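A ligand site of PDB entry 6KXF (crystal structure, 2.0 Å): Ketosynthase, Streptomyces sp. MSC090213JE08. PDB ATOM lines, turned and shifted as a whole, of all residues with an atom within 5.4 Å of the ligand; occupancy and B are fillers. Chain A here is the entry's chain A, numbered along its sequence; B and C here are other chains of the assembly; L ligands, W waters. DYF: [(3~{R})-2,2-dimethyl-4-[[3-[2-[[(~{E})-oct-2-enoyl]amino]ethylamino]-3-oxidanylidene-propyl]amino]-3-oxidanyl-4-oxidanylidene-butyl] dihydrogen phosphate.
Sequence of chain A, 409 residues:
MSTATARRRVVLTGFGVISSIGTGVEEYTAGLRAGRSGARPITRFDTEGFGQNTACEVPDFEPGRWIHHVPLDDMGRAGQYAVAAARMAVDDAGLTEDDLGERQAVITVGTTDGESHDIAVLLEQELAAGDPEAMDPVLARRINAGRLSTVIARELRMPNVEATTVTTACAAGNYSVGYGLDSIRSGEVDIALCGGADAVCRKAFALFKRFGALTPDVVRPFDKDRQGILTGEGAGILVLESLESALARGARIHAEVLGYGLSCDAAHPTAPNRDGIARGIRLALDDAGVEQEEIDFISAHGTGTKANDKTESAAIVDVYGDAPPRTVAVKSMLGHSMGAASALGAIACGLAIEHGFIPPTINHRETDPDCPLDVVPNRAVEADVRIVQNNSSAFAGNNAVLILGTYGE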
ATOM      1  N   THR A 112      20.346  30.139 -17.857  1.00  0.00           N
ATOM      2  CA  THR A 112      19.736  29.642 -19.055  1.00  0.00           C
ATOM      3  C   THR A 112      19.980  30.594 -20.232  1.00  0.00           C
ATOM      4  O   THR A 112      20.383  30.141 -21.262  1.00  0.00           O
ATOM      5  CB  THR A 112      18.216  29.492 -18.864  1.00  0.00           C
ATOM      6  OG1 THR A 112      17.980  28.547 -17.838  1.00  0.00           O
ATOM      7  CG2 THR A 112      17.507  29.028 -20.124  1.00  0.00           C
ATOM      8  N   ASP A 113      19.615  31.871 -20.062  1.00  0.00           N
ATOM      9  CA  ASP A 113      19.514  32.864 -21.133  1.00  0.00           C
ATOM     10  C   ASP A 113      20.590  33.950 -20.988  1.00  0.00           C
ATOM     11  O   ASP A 113      20.793  34.704 -21.908  1.00  0.00           O
ATOM     12  CB  ASP A 113      18.133  33.535 -21.148  1.00  0.00           C
ATOM     13  CG  ASP A 113      17.011  32.576 -21.592  1.00  0.00           C
ATOM     14  OD1 ASP A 113      17.241  31.823 -22.549  1.00  0.00           O
ATOM     15  OD2 ASP A 113      15.926  32.548 -20.920  1.00  0.00           O
ATOM     16  N   ALA A 169      21.062  25.409 -18.155  1.00  0.00           N
ATOM     17  CA  ALA A 169      19.736  25.926 -18.372  1.00  0.00           C
ATOM     18  C   ALA A 169      18.891  25.727 -17.098  1.00  0.00           C
ATOM     19  O   ALA A 169      19.243  26.214 -16.033  1.00  0.00           O
ATOM     20  CB  ALA A 169      19.157  25.262 -19.602  1.00  0.00           C
ATOM     21  N   CYS A 170      17.779  24.998 -17.189  1.00  0.00           N
ATOM     22  CA  CYS A 170      16.791  25.021 -16.150  1.00  0.00           C
ATOM     23  C   CYS A 170      17.204  24.158 -14.953  1.00  0.00           C
ATOM     24  O   CYS A 170      16.541  24.201 -13.978  1.00  0.00           O
ATOM     25  CB  CYS A 170      15.451  24.620 -16.757  1.00  0.00           C
ATOM     26  SG  CYS A 170      14.897  25.922 -17.877  1.00  0.00           S
ATOM     27  N   LYS A 203      12.986  36.434 -25.723  1.00  0.00           N
ATOM     28  CA  LYS A 203      13.331  35.117 -26.264  1.00  0.00           C
ATOM     29  C   LYS A 203      12.593  34.011 -25.500  1.00  0.00           C
ATOM     30  O   LYS A 203      11.971  33.130 -26.128  1.00  0.00           O
ATOM     31  CB  LYS A 203      14.835  34.870 -26.237  1.00  0.00           C
ATOM     32  CG  LYS A 203      15.304  33.519 -26.764  1.00  0.00           C
ATOM     33  CD  LYS A 203      16.573  33.114 -26.058  1.00  0.00           C
ATOM     34  CE  LYS A 203      17.112  31.728 -26.363  1.00  0.00           C
ATOM     35  NZ  LYS A 203      18.311  31.508 -25.529  1.00  0.00           N
ATOM     36  N   LEU A 207       9.694  31.579 -26.972  1.00  0.00           N
ATOM     37  CA  LEU A 207      10.060  30.178 -26.979  1.00  0.00           C
ATOM     38  C   LEU A 207       8.907  29.351 -26.399  1.00  0.00           C
ATOM     39  O   LEU A 207       8.390  28.388 -27.040  1.00  0.00           O
ATOM     40  CB  LEU A 207      11.335  29.967 -26.149  1.00  0.00           C
ATOM     41  CG  LEU A 207      12.036  28.613 -26.251  1.00  0.00           C
ATOM     42  CD1 LEU A 207      13.499  28.738 -25.820  1.00  0.00           C
ATOM     43  CD2 LEU A 207      11.359  27.526 -25.423  1.00  0.00           C
ATOM     44  N   PHE A 208       8.500  29.714 -25.179  1.00  0.00           N
ATOM     45  CA  PHE A 208       7.470  28.923 -24.491  1.00  0.00           C
ATOM     46  C   PHE A 208       6.146  29.070 -25.228  1.00  0.00           C
ATOM     47  O   PHE A 208       5.410  28.102 -25.334  1.00  0.00           O
ATOM     48  CB  PHE A 208       7.391  29.267 -22.997  1.00  0.00           C
ATOM     49  CG  PHE A 208       8.412  28.467 -22.236  1.00  0.00           C
ATOM     50  CD1 PHE A 208       8.153  27.137 -21.902  1.00  0.00           C
ATOM     51  CD2 PHE A 208       9.671  28.971 -21.959  1.00  0.00           C
ATOM     52  CE1 PHE A 208       9.092  26.373 -21.242  1.00  0.00           C
ATOM     53  CE2 PHE A 208      10.620  28.204 -21.298  1.00  0.00           C
ATOM     54  CZ  PHE A 208      10.325  26.907 -20.940  1.00  0.00           C
ATOM     55  N   PHE A 211       6.128  26.699 -28.152  1.00  0.00           N
ATOM     56  CA  PHE A 211       6.009  25.294 -27.758  1.00  0.00           C
ATOM     57  C   PHE A 211       4.644  24.988 -27.105  1.00  0.00           C
ATOM     58  O   PHE A 211       4.390  23.859 -26.709  1.00  0.00           O
ATOM     59  CB  PHE A 211       7.157  24.886 -26.831  1.00  0.00           C
ATOM     60  CG  PHE A 211       8.428  24.376 -27.476  1.00  0.00           C
ATOM     61  CD1 PHE A 211       8.541  24.136 -28.835  1.00  0.00           C
ATOM     62  CD2 PHE A 211       9.520  24.089 -26.676  1.00  0.00           C
ATOM     63  CE1 PHE A 211       9.714  23.649 -29.400  1.00  0.00           C
ATOM     64  CE2 PHE A 211      10.702  23.600 -27.230  1.00  0.00           C
ATOM     65  CZ  PHE A 211      10.788  23.378 -28.583  1.00  0.00           C
ATOM     66  N   ALA A 213       3.564  26.006 -24.212  1.00  0.00           N
ATOM     67  CA  ALA A 213       3.846  25.671 -22.824  1.00  0.00           C
ATOM     68  C   ALA A 213       3.762  26.911 -21.920  1.00  0.00           C
ATOM     69  O   ALA A 213       4.217  26.905 -20.810  1.00  0.00           O
ATOM     70  CB  ALA A 213       5.207  25.032 -22.743  1.00  0.00           C
ATOM     71  N   HIS A 268      15.961  12.293 -25.463  1.00  0.00           N
ATOM     72  CA  HIS A 268      15.327  13.275 -26.267  1.00  0.00           C
ATOM     73  C   HIS A 268      15.913  14.662 -25.962  1.00  0.00           C
ATOM     74  O   HIS A 268      16.383  14.912 -24.845  1.00  0.00           O
ATOM     75  CB  HIS A 268      13.821  13.221 -25.974  1.00  0.00           C
ATOM     76  CG  HIS A 268      12.990  13.865 -27.036  1.00  0.00           C
ATOM     77  ND1 HIS A 268      12.773  15.223 -27.062  1.00  0.00           N
ATOM     78  CD2 HIS A 268      12.345  13.335 -28.103  1.00  0.00           C
ATOM     79  CE1 HIS A 268      12.003  15.519 -28.097  1.00  0.00           C
ATOM     80  NE2 HIS A 268      11.717  14.367 -28.750  1.00  0.00           N
ATOM     81  N   THR A 270      14.310  17.689 -25.715  1.00  0.00           N
ATOM     82  CA  THR A 270      13.426  18.586 -24.991  1.00  0.00           C
ATOM     83  C   THR A 270      12.529  17.843 -23.993  1.00  0.00           C
ATOM     84  O   THR A 270      12.133  18.427 -22.985  1.00  0.00           O
ATOM     85  CB  THR A 270      12.591  19.457 -25.945  1.00  0.00           C
ATOM     86  OG1 THR A 270      11.617  18.639 -26.620  1.00  0.00           O
ATOM     87  CG2 THR A 270      13.445  20.245 -26.921  1.00  0.00           C
ATOM     88  N   ALA A 271      12.199  16.574 -24.256  1.00  0.00           N
ATOM     89  CA  ALA A 271      11.280  15.824 -23.441  1.00  0.00           C
ATOM     90  C   ALA A 271      12.001  15.358 -22.193  1.00  0.00           C
ATOM     91  O   ALA A 271      13.149  14.943 -22.273  1.00  0.00           O
ATOM     92  CB  ALA A 271      10.742  14.620 -24.192  1.00  0.00           C
ATOM     93  N   PRO A 272      11.336  15.364 -21.013  1.00  0.00           N
ATOM     94  CA  PRO A 272      11.934  14.804 -19.807  1.00  0.00           C
ATOM     95  C   PRO A 272      11.845  13.275 -19.873  1.00  0.00           C
ATOM     96  O   PRO A 272      11.066  12.773 -20.611  1.00  0.00           O
ATOM     97  CB  PRO A 272      11.054  15.343 -18.686  1.00  0.00           C
ATOM     98  CG  PRO A 272       9.707  15.513 -19.347  1.00  0.00           C
ATOM     99  CD  PRO A 272      10.022  15.973 -20.754  1.00  0.00           C
ATOM    100  N   HIS A 301      10.815  19.935  -9.510  1.00  0.00           N
ATOM    101  CA  HIS A 301      11.094  20.834 -10.578  1.00  0.00           C
ATOM    102  C   HIS A 301       9.788  21.473 -11.047  1.00  0.00           C
ATOM    103  O   HIS A 301       9.729  22.694 -11.218  1.00  0.00           O
ATOM    104  CB  HIS A 301      11.870  20.137 -11.703  1.00  0.00           C
ATOM    105  CG  HIS A 301      12.279  21.094 -12.765  1.00  0.00           C
ATOM    106  ND1 HIS A 301      13.193  22.115 -12.538  1.00  0.00           N
ATOM    107  CD2 HIS A 301      11.900  21.222 -14.062  1.00  0.00           C
ATOM    108  CE1 HIS A 301      13.388  22.795 -13.653  1.00  0.00           C
ATOM    109  NE2 HIS A 301      12.624  22.253 -14.608  1.00  0.00           N
ATOM    110  N   THR A 303       7.219  22.414 -13.241  1.00  0.00           N
ATOM    111  CA  THR A 303       7.059  23.607 -14.054  1.00  0.00           C
ATOM    112  C   THR A 303       5.604  23.902 -14.393  1.00  0.00           C
ATOM    113  O   THR A 303       5.282  25.041 -14.832  1.00  0.00           O
ATOM    114  CB  THR A 303       7.846  23.497 -15.365  1.00  0.00           C
ATOM    115  OG1 THR A 303       7.449  22.282 -16.012  1.00  0.00           O
ATOM    116  CG2 THR A 303       9.342  23.537 -15.144  1.00  0.00           C
ATOM    117  N   THR A 305       4.008  22.211 -16.777  1.00  0.00           N
ATOM    118  CA  THR A 305       3.702  21.692 -18.137  1.00  0.00           C
ATOM    119  C   THR A 305       3.075  20.291 -18.030  1.00  0.00           C
ATOM    120  O   THR A 305       3.224  19.561 -17.031  1.00  0.00           O
ATOM    121  CB  THR A 305       4.933  21.652 -19.061  1.00  0.00           C
ATOM    122  OG1 THR A 305       5.927  20.758 -18.556  1.00  0.00           O
ATOM    123  CG2 THR A 305       5.568  23.001 -19.273  1.00  0.00           C
ATOM    124  N   ALA A 307       3.922  17.625 -19.831  1.00  0.00           N
ATOM    125  CA  ALA A 307       4.946  16.587 -19.924  1.00  0.00           C
ATOM    126  C   ALA A 307       5.772  16.564 -18.638  1.00  0.00           C
ATOM    127  O   ALA A 307       6.108  15.496 -18.155  1.00  0.00           O
ATOM    128  CB  ALA A 307       5.824  16.824 -21.119  1.00  0.00           C
ATOM    129  N   ASN A 308       6.109  17.746 -18.094  1.00  0.00           N
ATOM    130  CA  ASN A 308       7.046  17.734 -16.940  1.00  0.00           C
ATOM    131  C   ASN A 308       6.414  17.014 -15.739  1.00  0.00           C
ATOM    132  O   ASN A 308       7.004  16.124 -15.149  1.00  0.00           O
ATOM    133  CB  ASN A 308       7.484  19.113 -16.446  1.00  0.00           C
ATOM    134  CG  ASN A 308       8.322  18.970 -15.188  1.00  0.00           C
ATOM    135  OD1 ASN A 308       9.489  18.621 -15.283  1.00  0.00           O
ATOM    136  ND2 ASN A 308       7.701  19.098 -14.015  1.00  0.00           N
ATOM    137  N   HIS A 336       8.628  30.333 -13.670  1.00  0.00           N
ATOM    138  CA  HIS A 336       9.867  29.605 -14.004  1.00  0.00           C
ATOM    139  C   HIS A 336      11.009  30.622 -14.139  1.00  0.00           C
ATOM    140  O   HIS A 336      11.129  31.298 -15.150  1.00  0.00           O
ATOM    141  CB  HIS A 336       9.675  28.739 -15.261  1.00  0.00           C
ATOM    142  CG  HIS A 336      10.734  27.704 -15.472  1.00  0.00           C
ATOM    143  ND1 HIS A 336      11.992  27.811 -14.926  1.00  0.00           N
ATOM    144  CD2 HIS A 336      10.754  26.596 -16.233  1.00  0.00           C
ATOM    145  CE1 HIS A 336      12.720  26.766 -15.267  1.00  0.00           C
ATOM    146  NE2 HIS A 336      11.987  26.005 -16.098  1.00  0.00           N
ATOM    147  N   MET A 338      14.059  29.957 -14.590  1.00  0.00           N
ATOM    148  CA  MET A 338      15.066  29.500 -15.536  1.00  0.00           C
ATOM    149  C   MET A 338      16.309  28.993 -14.752  1.00  0.00           C
ATOM    150  O   MET A 338      16.171  28.090 -13.933  1.00  0.00           O
ATOM    151  CB  MET A 338      15.391  30.641 -16.522  1.00  0.00           C
ATOM    152  CG  MET A 338      14.140  31.143 -17.256  1.00  0.00           C
ATOM    153  SD  MET A 338      13.262  29.744 -18.131  1.00  0.00           S
ATOM    154  CE  MET A 338      11.752  30.633 -18.511  1.00  0.00           C
ATOM    155  N   SER A 393      15.583  19.801 -13.619  1.00  0.00           N
ATOM    156  CA  SER A 393      15.931  19.172 -14.860  1.00  0.00           C
ATOM    157  C   SER A 393      15.797  20.212 -15.988  1.00  0.00           C
ATOM    158  O   SER A 393      15.303  21.328 -15.794  1.00  0.00           O
ATOM    159  CB  SER A 393      15.120  17.902 -15.105  1.00  0.00           C
ATOM    160  OG  SER A 393      13.897  18.207 -15.717  1.00  0.00           O
ATOM    161  N   ALA A 394      16.336  19.858 -17.147  1.00  0.00           N
ATOM    162  CA  ALA A 394      16.433  20.805 -18.236  1.00  0.00           C
ATOM    163  C   ALA A 394      16.333  20.083 -19.598  1.00  0.00           C
ATOM    164  O   ALA A 394      16.376  18.862 -19.641  1.00  0.00           O
ATOM    165  CB  ALA A 394      17.762  21.509 -18.102  1.00  0.00           C
ATOM    166  N   PHE A 395      16.220  20.871 -20.681  1.00  0.00           N
ATOM    167  CA  PHE A 395      16.465  20.357 -22.013  1.00  0.00           C
ATOM    168  C   PHE A 395      17.846  19.704 -22.049  1.00  0.00           C
ATOM    169  O   PHE A 395      18.653  19.860 -21.094  1.00  0.00           O
ATOM    170  CB  PHE A 395      16.329  21.466 -23.057  1.00  0.00           C
ATOM    171  CG  PHE A 395      14.937  22.036 -23.215  1.00  0.00           C
ATOM    172  CD1 PHE A 395      13.825  21.437 -22.633  1.00  0.00           C
ATOM    173  CD2 PHE A 395      14.736  23.171 -23.985  1.00  0.00           C
ATOM    174  CE1 PHE A 395      12.561  21.983 -22.777  1.00  0.00           C
ATOM    175  CE2 PHE A 395      13.458  23.687 -24.168  1.00  0.00           C
ATOM    176  CZ  PHE A 395      12.375  23.092 -23.563  1.00  0.00           C
ATOM    177  N   ASP B  40       6.609  12.448 -33.554  1.00  0.00           N
ATOM    178  CA  ASP B  40       7.307  13.110 -32.465  1.00  0.00           C
ATOM    179  C   ASP B  40       6.518  14.395 -32.213  1.00  0.00           C
ATOM    180  O   ASP B  40       6.169  15.090 -33.177  1.00  0.00           O
ATOM    181  CB  ASP B  40       8.766  13.433 -32.808  1.00  0.00           C
ATOM    182  CG  ASP B  40       9.644  13.834 -31.628  1.00  0.00           C
ATOM    183  OD1 ASP B  40       9.898  12.972 -30.768  1.00  0.00           O
ATOM    184  OD2 ASP B  40      10.070  15.008 -31.600  1.00  0.00           O
ATOM    185  N   SER B  41       6.194  14.667 -30.936  1.00  0.00           N
ATOM    186  CA  SER B  41       5.371  15.835 -30.565  1.00  0.00           C
ATOM    187  C   SER B  41       6.000  17.143 -31.086  1.00  0.00           C
ATOM    188  O   SER B  41       5.266  18.095 -31.372  1.00  0.00           O
ATOM    189  CB  SER B  41       5.154  15.894 -29.077  1.00  0.00           C
ATOM    190  N   LEU B  42       7.341  17.160 -31.210  1.00  0.00           N
ATOM    191  CA  LEU B  42       8.104  18.281 -31.791  1.00  0.00           C
ATOM    192  C   LEU B  42       7.791  18.378 -33.291  1.00  0.00           C
ATOM    193  O   LEU B  42       7.728  19.470 -33.823  1.00  0.00           O
ATOM    194  CB  LEU B  42       9.617  18.053 -31.625  1.00  0.00           C
ATOM    195  CG  LEU B  42      10.260  18.557 -30.334  1.00  0.00           C
ATOM    196  CD1 LEU B  42      11.782  18.545 -30.459  1.00  0.00           C
ATOM    197  CD2 LEU B  42       9.779  19.953 -29.964  1.00  0.00           C
ATOM    198  N   ILE B  45       4.484  20.009 -33.710  1.00  0.00           N
ATOM    199  CA  ILE B  45       4.594  21.445 -33.401  1.00  0.00           C
ATOM    200  C   ILE B  45       5.243  22.150 -34.600  1.00  0.00           C
ATOM    201  O   ILE B  45       4.810  23.239 -35.003  1.00  0.00           O
ATOM    202  CB  ILE B  45       5.348  21.683 -32.066  1.00  0.00           C
ATOM    203  CG1 ILE B  45       4.449  21.371 -30.856  1.00  0.00           C
ATOM    204  CG2 ILE B  45       5.915  23.091 -31.996  1.00  0.00           C
ATOM    205  CD1 ILE B  45       5.208  21.052 -29.589  1.00  0.00           C
ATOM    206  N   ILE C 149      14.681  25.607 -32.085  1.00  0.00           N
ATOM    207  CA  ILE C 149      14.665  26.001 -30.661  1.00  0.00           C
ATOM    208  C   ILE C 149      15.594  25.116 -29.839  1.00  0.00           C
ATOM    209  O   ILE C 149      16.386  25.637 -29.081  1.00  0.00           O
ATOM    210  CB  ILE C 149      13.232  26.060 -30.109  1.00  0.00           C
ATOM    211  CG1 ILE C 149      12.561  27.356 -30.584  1.00  0.00           C
ATOM    212  CG2 ILE C 149      13.211  25.933 -28.586  1.00  0.00           C
ATOM    213  CD1 ILE C 149      11.039  27.307 -30.594  1.00  0.00           C
ATOM    214  N   GLY C 152      19.225  26.074 -29.928  1.00  0.00           N
ATOM    215  CA  GLY C 152      19.574  27.343 -29.280  1.00  0.00           C
ATOM    216  C   GLY C 152      20.045  27.200 -27.822  1.00  0.00           C
ATOM    217  O   GLY C 152      20.697  28.095 -27.324  1.00  0.00           O
ATOM    218  N   SER C 153      19.712  26.092 -27.143  1.00  0.00           N
ATOM    219  CA  SER C 153      20.119  25.909 -25.758  1.00  0.00           C
ATOM    220  C   SER C 153      21.637  25.891 -25.681  1.00  0.00           C
ATOM    221  O   SER C 153      22.284  25.211 -26.467  1.00  0.00           O
ATOM    222  CB  SER C 153      19.582  24.634 -25.142  1.00  0.00           C
ATOM    223  OG  SER C 153      18.185  24.666 -25.138  1.00  0.00           O
HETATM  224  C29 DYF L   1      14.988  27.026 -22.722  1.00  0.00           C
HETATM  225  C26 DYF L   1      13.856  25.283 -19.372  1.00  0.00           C
HETATM  226  C25 DYF L   1      13.028  24.234 -19.508  1.00  0.00           C
HETATM  227  O13 DYF L   1       6.923  20.161 -22.736  1.00  0.00           O
HETATM  228  C21 DYF L   1      12.820  20.749 -18.564  1.00  0.00           C
HETATM  229  C17 DYF L   1       9.237  20.650 -19.248  1.00  0.00           C
HETATM  230  O11 DYF L   1       8.684  18.152 -25.072  1.00  0.00           O
HETATM  231  N22 DYF L   1      12.915  21.969 -17.994  1.00  0.00           N
HETATM  232  C10 DYF L   1       7.520  18.874 -24.679  1.00  0.00           C
HETATM  233  N19 DYF L   1      10.525  20.097 -18.959  1.00  0.00           N
HETATM  234  C30 DYF L   1      16.439  27.227 -23.196  1.00  0.00           C
HETATM  235  C31 DYF L   1      16.643  28.125 -24.422  1.00  0.00           C
HETATM  236  N14 DYF L   1       9.144  19.703 -22.918  1.00  0.00           N
HETATM  237  C28 DYF L   1      14.949  25.960 -21.607  1.00  0.00           C
HETATM  238  C27 DYF L   1      14.061  26.369 -20.444  1.00  0.00           C
HETATM  239  C23 DYF L   1      12.860  23.316 -18.277  1.00  0.00           C
HETATM  240  C20 DYF L   1      11.421  20.444 -17.883  1.00  0.00           C
HETATM  241  C16 DYF L   1       8.685  19.998 -20.496  1.00  0.00           C
HETATM  242  C15 DYF L   1       9.473  20.434 -21.717  1.00  0.00           C
HETATM  243  C12 DYF L   1       7.782  19.631 -23.376  1.00  0.00           C
HETATM  244  C01 DYF L   1       8.315  20.831 -26.134  1.00  0.00           C
HETATM  245  C02 DYF L   1       7.205  19.781 -25.902  1.00  0.00           C
HETATM  246  C03 DYF L   1       5.851  20.495 -25.778  1.00  0.00           C
HETATM  247  C04 DYF L   1       7.124  18.834 -27.131  1.00  0.00           C
HETATM  248  O05 DYF L   1       6.073  17.910 -26.936  1.00  0.00           O
HETATM  249  P06 DYF L   1       6.301  16.281 -26.732  1.00  0.00           P
HETATM  250  O07 DYF L   1       5.972  15.615 -28.050  1.00  0.00           O
HETATM  251  O08 DYF L   1       5.265  15.848 -25.705  1.00  0.00           O
HETATM  252  O09 DYF L   1       7.745  15.887 -26.526  1.00  0.00           O
HETATM  253  O18 DYF L   1       8.652  21.500 -18.614  1.00  0.00           O
HETATM  254  O24 DYF L   1      12.751  23.676 -17.121  1.00  0.00           O
HETATM  255  O   HOH W   1       4.396  19.617 -22.044  1.00  0.00           O
HETATM  256  O   HOH W   2      16.458  23.640 -20.285  1.00  0.00           O
HETATM  257  O   HOH W   3      12.420  18.545 -20.308  1.00  0.00           O
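Water W1 lies within hydrogen-bond range of O13 of the ligand (2.7 Å) and N of Ala 307 (3.0 Å).
Water W3 lies within hydrogen-bond range of the backbone carbonyl oxygen (O) of Thr 270 (2.7 Å) and a nitrogen (N19) of the ligand (2.8 Å).
Water W2 lies within hydrogen-bond range of N of Phe 395 and SG of Cys 170.
Thr 112 touches the ligand (CG2 to C30, 3.7 Å).
NZ of Lys 203 touches C31 of the ligand, 3.9 Å away.
CD1 of Leu 207 touches C31 of the ligand (3.5 Å).
Phe 208 touches the ligand (CZ to C27, 3.8 Å).
Phe 211 touches the ligand (CD2 to C01, 3.5 Å).
CA of Ala 271 touches O11 of the ligand, 3.8 Å away.
Ala 307 touches the ligand (CB to O13, 3.9 Å).
Asn 308 touches the ligand.
Ala 394 touches the ligand.
Phe 395 touches the ligand.
N of Leu 42 of chain B touches O07 of the ligand, 3.8 Å away.
Ile 45 of chain B touches the ligand (CD1 to C04, 3.8 Å).
Ser 153 of chain C touches the ligand.
An oxygen (O11) of the ligand sits at hydrogen-bond distance from the side-chain hydroxyl of Thr 270, 3.4 Å away.
OG1 of Thr 303 is in hydrogen-bond range of O18 of the ligand (3.0 Å).
The side-chain hydroxyl of Thr 305 lies within hydrogen-bond range of an oxygen (O18) of the ligand (2.8 Å).
O of Ser 393 lies within hydrogen-bond range of N22 of the ligand (3.3 Å).
O of Thr 270 is in hydrogen-bond range of N14 of the ligand.
A ring nitrogen (NE2) of His 336 is in hydrogen-bond range of an oxygen (O24) of the ligand, at 2.7 Å.
CB of Ser 41 of chain B is bonded to O07 of the ligand (1.3 Å).
The side-chain sulfur (SG) of Cys 170 is bonded to a carbon (C26) of the ligand, at 1.9 Å.
O24 of the ligand lies within hydrogen-bond range of NE2 of His 301 (2.9 Å).
The backbone NH of Ser 41 of chain B sits close to an oxygen (O07) of the ligand (3.0 Å).
The backbone carbonyl oxygen (O) of Phe 208 lies within hydrogen-bond range of the backbone NH (N) of Ala 213, 3.0 Å away.
N of Leu 42 of chain B sits close to OD2 of Asp 40 of chain B (3.5 Å).
The backbone NH (N) of Thr 303 lies close to the side-chain amide nitrogen (ND2) of Asn 308 (3.4 Å).
The backbone NH (N) of Ala 271 lies within hydrogen-bond range of a ring nitrogen (ND1) of His 268.
The side-chain hydroxyl of Thr 305 sits at hydrogen-bond distance from the backbone NH of Asn 308 (3.1 Å).
ND1 of His 336 sits at hydrogen-bond distance from N of Met 338, 3.0 Å away.
A ring nitrogen (ND1) of His 268 is in hydrogen-bond range of the backbone NH (N) of Thr 270 (3.2 Å).
OG1 of Thr 112 lies close to O of Ala 169.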
